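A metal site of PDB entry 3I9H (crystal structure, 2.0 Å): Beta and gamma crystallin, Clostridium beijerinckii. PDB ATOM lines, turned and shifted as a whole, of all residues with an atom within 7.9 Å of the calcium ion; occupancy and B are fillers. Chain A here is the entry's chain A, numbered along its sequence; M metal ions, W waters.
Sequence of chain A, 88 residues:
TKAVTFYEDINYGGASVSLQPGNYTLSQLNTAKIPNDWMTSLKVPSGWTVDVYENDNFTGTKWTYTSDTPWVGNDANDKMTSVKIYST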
ATOM      1  N   TYR A   7     -21.416   3.783 -26.028  1.00  0.00           N
ATOM      2  CA  TYR A   7     -21.854   4.193 -24.696  1.00  0.00           C
ATOM      3  C   TYR A   7     -23.300   3.820 -24.412  1.00  0.00           C
ATOM      4  O   TYR A   7     -24.132   3.808 -25.315  1.00  0.00           O
ATOM      5  CB  TYR A   7     -21.720   5.705 -24.524  1.00  0.00           C
ATOM      6  CG  TYR A   7     -20.308   6.207 -24.623  1.00  0.00           C
ATOM      7  CD1 TYR A   7     -19.711   6.410 -25.863  1.00  0.00           C
ATOM      8  CD2 TYR A   7     -19.558   6.470 -23.474  1.00  0.00           C
ATOM      9  CE1 TYR A   7     -18.391   6.869 -25.966  1.00  0.00           C
ATOM     10  CE2 TYR A   7     -18.249   6.926 -23.564  1.00  0.00           C
ATOM     11  CZ  TYR A   7     -17.671   7.119 -24.798  1.00  0.00           C
ATOM     12  OH  TYR A   7     -16.361   7.537 -24.880  1.00  0.00           O
ATOM     13  N   GLU A   8     -23.566   3.525 -23.148  1.00  0.00           N
ATOM     14  CA  GLU A   8     -24.898   3.155 -22.702  1.00  0.00           C
ATOM     15  C   GLU A   8     -25.873   4.318 -22.808  1.00  0.00           C
ATOM     16  O   GLU A   8     -26.987   4.159 -23.267  1.00  0.00           O
ATOM     17  CB  GLU A   8     -24.858   2.650 -21.246  1.00  0.00           C
ATOM     18  CG  GLU A   8     -26.233   2.507 -20.602  1.00  0.00           C
ATOM     19  CD  GLU A   8     -26.156   2.063 -19.143  1.00  0.00           C
ATOM     20  OE1 GLU A   8     -25.143   2.355 -18.476  1.00  0.00           O
ATOM     21  OE2 GLU A   8     -27.116   1.419 -18.673  1.00  0.00           O
ATOM     22  N   ASP A   9     -25.433   5.508 -22.425  1.00  0.00           N
ATOM     23  CA  ASP A   9     -26.315   6.664 -22.458  1.00  0.00           C
ATOM     24  C   ASP A   9     -25.978   7.749 -23.474  1.00  0.00           C
ATOM     25  O   ASP A   9     -24.938   7.725 -24.136  1.00  0.00           O
ATOM     26  CB  ASP A   9     -26.398   7.296 -21.067  1.00  0.00           C
ATOM     27  CG  ASP A   9     -26.992   6.341 -20.043  1.00  0.00           C
ATOM     28  OD1 ASP A   9     -28.050   5.750 -20.342  1.00  0.00           O
ATOM     29  OD2 ASP A   9     -26.406   6.201 -18.953  1.00  0.00           O
ATOM     30  N   ILE A  10     -26.902   8.696 -23.589  1.00  0.00           N
ATOM     31  CA  ILE A  10     -26.755   9.813 -24.504  1.00  0.00           C
ATOM     32  C   ILE A  10     -25.591  10.682 -24.012  1.00  0.00           C
ATOM     33  O   ILE A  10     -25.287  10.693 -22.819  1.00  0.00           O
ATOM     34  CB  ILE A  10     -28.050  10.647 -24.544  1.00  0.00           C
ATOM     35  CG1 ILE A  10     -27.948  11.736 -25.606  1.00  0.00           C
ATOM     36  CG2 ILE A  10     -28.343  11.231 -23.170  1.00  0.00           C
ATOM     37  CD1 ILE A  10     -29.272  12.411 -25.917  1.00  0.00           C
ATOM     38  N   GLY A  13     -22.568   8.949 -21.984  1.00  0.00           N
ATOM     39  CA  GLY A  13     -22.682   8.704 -20.555  1.00  0.00           C
ATOM     40  C   GLY A  13     -22.910   7.239 -20.243  1.00  0.00           C
ATOM     41  O   GLY A  13     -23.045   6.418 -21.152  1.00  0.00           O
ATOM     42  N   ASN A  36     -27.469  -6.411 -25.379  1.00  0.00           N
ATOM     43  CA  ASN A  36     -28.327  -6.218 -26.539  1.00  0.00           C
ATOM     44  C   ASN A  36     -29.172  -4.950 -26.319  1.00  0.00           C
ATOM     45  O   ASN A  36     -29.429  -4.567 -25.180  1.00  0.00           O
ATOM     46  CB  ASN A  36     -29.251  -7.439 -26.694  1.00  0.00           C
ATOM     47  CG  ASN A  36     -29.826  -7.557 -28.091  1.00  0.00           C
ATOM     48  OD1 ASN A  36     -29.528  -6.747 -28.962  1.00  0.00           O
ATOM     49  ND2 ASN A  36     -30.654  -8.582 -28.301  1.00  0.00           N
ATOM     50  N   ASP A  37     -29.579  -4.317 -27.421  1.00  0.00           N
ATOM     51  CA  ASP A  37     -30.428  -3.111 -27.375  1.00  0.00           C
ATOM     52  C   ASP A  37     -30.045  -2.197 -26.224  1.00  0.00           C
ATOM     53  O   ASP A  37     -30.850  -1.922 -25.331  1.00  0.00           O
ATOM     54  CB  ASP A  37     -31.881  -3.542 -27.255  1.00  0.00           C
ATOM     55  CG  ASP A  37     -32.257  -4.580 -28.283  1.00  0.00           C
ATOM     56  OD1 ASP A  37     -31.768  -4.432 -29.416  1.00  0.00           O
ATOM     57  OD2 ASP A  37     -33.009  -5.531 -27.980  1.00  0.00           O
ATOM     58  N   TRP A  38     -28.825  -1.683 -26.287  1.00  0.00           N
ATOM     59  CA  TRP A  38     -28.265  -0.853 -25.227  1.00  0.00           C
ATOM     60  C   TRP A  38     -27.477   0.369 -25.706  1.00  0.00           C
ATOM     61  O   TRP A  38     -27.305   1.326 -24.966  1.00  0.00           O
ATOM     62  CB  TRP A  38     -27.377  -1.788 -24.397  1.00  0.00           C
ATOM     63  CG  TRP A  38     -26.329  -1.175 -23.529  1.00  0.00           C
ATOM     64  CD1 TRP A  38     -26.380  -1.024 -22.166  1.00  0.00           C
ATOM     65  CD2 TRP A  38     -25.019  -0.756 -23.930  1.00  0.00           C
ATOM     66  NE1 TRP A  38     -25.183  -0.549 -21.704  1.00  0.00           N
ATOM     67  CE2 TRP A  38     -24.326  -0.373 -22.760  1.00  0.00           C
ATOM     68  CE3 TRP A  38     -24.369  -0.656 -25.167  1.00  0.00           C
ATOM     69  CZ2 TRP A  38     -23.002   0.096 -22.779  1.00  0.00           C
ATOM     70  CZ3 TRP A  38     -23.047  -0.200 -25.197  1.00  0.00           C
ATOM     71  CH2 TRP A  38     -22.383   0.170 -24.007  1.00  0.00           C
ATOM     72  N   MET A  39     -26.997   0.332 -26.951  1.00  0.00           N
ATOM     73  CA  MET A  39     -26.207   1.446 -27.473  1.00  0.00           C
ATOM     74  C   MET A  39     -27.029   2.710 -27.729  1.00  0.00           C
ATOM     75  O   MET A  39     -28.063   2.660 -28.395  1.00  0.00           O
ATOM     76  CB  MET A  39     -25.481   0.993 -28.750  1.00  0.00           C
ATOM     77  CG  MET A  39     -24.321   1.873 -29.170  1.00  0.00           C
ATOM     78  SD  MET A  39     -24.857   3.295 -30.104  1.00  0.00           S
ATOM     79  CE  MET A  39     -25.120   2.545 -31.727  1.00  0.00           C
ATOM     80  N   THR A  40     -26.561   3.830 -27.181  1.00  0.00           N
ATOM     81  CA  THR A  40     -27.240   5.116 -27.335  1.00  0.00           C
ATOM     82  C   THR A  40     -26.354   6.174 -28.003  1.00  0.00           C
ATOM     83  O   THR A  40     -26.862   7.062 -28.683  1.00  0.00           O
ATOM     84  CB  THR A  40     -27.729   5.632 -25.975  1.00  0.00           C
ATOM     85  OG1 THR A  40     -28.797   4.801 -25.529  1.00  0.00           O
ATOM     86  CG2 THR A  40     -28.233   7.073 -26.078  1.00  0.00           C
ATOM     87  N   SER A  41     -25.047   6.090 -27.775  1.00  0.00           N
ATOM     88  CA  SER A  41     -24.103   7.025 -28.390  1.00  0.00           C
ATOM     89  C   SER A  41     -22.791   6.284 -28.645  1.00  0.00           C
ATOM     90  O   SER A  41     -22.558   5.218 -28.079  1.00  0.00           O
ATOM     91  CB  SER A  41     -23.878   8.253 -27.503  1.00  0.00           C
ATOM     92  OG  SER A  41     -23.446   7.910 -26.199  1.00  0.00           O
ATOM     93  N   TRP A  71     -25.889  11.223 -29.830  1.00  0.00           N
ATOM     94  CA  TRP A  71     -27.276  10.792 -29.712  1.00  0.00           C
ATOM     95  C   TRP A  71     -27.635  10.111 -31.028  1.00  0.00           C
ATOM     96  O   TRP A  71     -27.767  10.764 -32.064  1.00  0.00           O
ATOM     97  CB  TRP A  71     -28.166  12.009 -29.470  1.00  0.00           C
ATOM     98  CG  TRP A  71     -29.673  11.786 -29.394  1.00  0.00           C
ATOM     99  CD1 TRP A  71     -30.633  12.681 -29.778  1.00  0.00           C
ATOM    100  CD2 TRP A  71     -30.376  10.641 -28.895  1.00  0.00           C
ATOM    101  NE1 TRP A  71     -31.886  12.168 -29.543  1.00  0.00           N
ATOM    102  CE2 TRP A  71     -31.761  10.916 -29.002  1.00  0.00           C
ATOM    103  CE3 TRP A  71     -29.980   9.397 -28.372  1.00  0.00           C
ATOM    104  CZ2 TRP A  71     -32.743  10.000 -28.605  1.00  0.00           C
ATOM    105  CZ3 TRP A  71     -30.963   8.496 -27.973  1.00  0.00           C
ATOM    106  CH2 TRP A  71     -32.328   8.803 -28.095  1.00  0.00           C
ATOM    107  N   VAL A  72     -27.764   8.790 -31.011  1.00  0.00           N
ATOM    108  CA  VAL A  72     -28.101   8.070 -32.233  1.00  0.00           C
ATOM    109  C   VAL A  72     -29.546   8.325 -32.663  1.00  0.00           C
ATOM    110  O   VAL A  72     -29.914   7.996 -33.781  1.00  0.00           O
ATOM    111  CB  VAL A  72     -27.899   6.548 -32.076  1.00  0.00           C
ATOM    112  CG1 VAL A  72     -26.410   6.236 -31.881  1.00  0.00           C
ATOM    113  CG2 VAL A  72     -28.714   6.031 -30.910  1.00  0.00           C
ATOM    114  N   ASN A  77     -31.864   4.133 -31.455  1.00  0.00           N
ATOM    115  CA  ASN A  77     -31.589   3.923 -30.041  1.00  0.00           C
ATOM    116  C   ASN A  77     -31.984   2.544 -29.491  1.00  0.00           C
ATOM    117  O   ASN A  77     -33.041   2.013 -29.805  1.00  0.00           O
ATOM    118  CB  ASN A  77     -32.259   4.999 -29.177  1.00  0.00           C
ATOM    119  CG  ASN A  77     -31.801   4.933 -27.737  1.00  0.00           C
ATOM    120  OD1 ASN A  77     -30.598   5.011 -27.456  1.00  0.00           O
ATOM    121  ND2 ASN A  77     -32.750   4.767 -26.818  1.00  0.00           N
ATOM    122  N   ASP A  78     -31.112   2.001 -28.648  1.00  0.00           N
ATOM    123  CA  ASP A  78     -31.329   0.702 -28.024  1.00  0.00           C
ATOM    124  C   ASP A  78     -31.748  -0.383 -28.999  1.00  0.00           C
ATOM    125  O   ASP A  78     -32.638  -1.192 -28.688  1.00  0.00           O
ATOM    126  CB  ASP A  78     -32.378   0.829 -26.913  1.00  0.00           C
ATOM    127  CG  ASP A  78     -31.876   1.645 -25.739  1.00  0.00           C
ATOM    128  OD1 ASP A  78     -30.653   1.881 -25.714  1.00  0.00           O
ATOM    129  OD2 ASP A  78     -32.681   2.021 -24.846  1.00  0.00           O
ATOM    130  N   LYS A  79     -31.112  -0.424 -30.160  1.00  0.00           N
ATOM    131  CA  LYS A  79     -31.440  -1.440 -31.150  1.00  0.00           C
ATOM    132  C   LYS A  79     -30.253  -2.273 -31.615  1.00  0.00           C
ATOM    133  O   LYS A  79     -30.425  -3.320 -32.215  1.00  0.00           O
ATOM    134  CB  LYS A  79     -32.141  -0.803 -32.341  1.00  0.00           C
ATOM    135  CG  LYS A  79     -33.395  -0.036 -31.965  1.00  0.00           C
ATOM    136  CD  LYS A  79     -34.310   0.170 -33.158  1.00  0.00           C
ATOM    137  CE  LYS A  79     -34.894  -1.143 -33.642  1.00  0.00           C
ATOM    138  NZ  LYS A  79     -35.869  -0.958 -34.773  1.00  0.00           N
HETATM  139 CA    CA M   1     -29.128   2.901 -23.906  1.00  0.00          CA
HETATM  140  O   HOH W   1     -30.063   4.189 -21.504  1.00  0.00           O
HETATM  141  O   HOH W   2     -31.357   4.476 -23.822  1.00  0.00           O
HETATM  142  O   HOH W   3     -29.595   0.871 -22.324  1.00  0.00           O
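The side-chain carboxylate (OD2) of Asp 78 sits at hydrogen-bond distance from the side-chain amide nitrogen (ND2) of Asn 77 (3.4 Å).
O of Thr 40 sits at hydrogen-bond distance from N of Val 72, 3.0 Å away.
The backbone carbonyl oxygen (O) of Tyr 7 sits at hydrogen-bond distance from the backbone NH (N) of Thr 40, at 3.1 Å.
The side-chain hydroxyl (OG1) of Thr 40 sits close to the side-chain amide oxygen (OD1) of Asn 77, 2.6 Å away.
The backbone NH of Asp 78 sits at hydrogen-bond distance from the backbone carbonyl oxygen of Met 39.
Of the 16 residues printed, 4 come within 4 Å of the calcium ion.
The nearest printed residue that does not touch the calcium ion is Met 39 (4.4 Å).
OG1 of Thr 40 binds the calcium ion (2.5 Å).
The calcium ion is bound by O of Glu 8.
The calcium ion is bound by the side-chain carboxylate (OD1) of Asp 78, at 2.6 Å.
Water W3 binds the calcium ion (2.6 Å).
O of Trp 38 binds the calcium ion (2.6 Å).
The calcium ion is bound by water W2, 2.7 Å away.
Water W1 binds the calcium ion.
Water W2 bridges OD2 of Asp 78 (3.0 Å) and ND2 of Asn 77 (3.3 Å).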
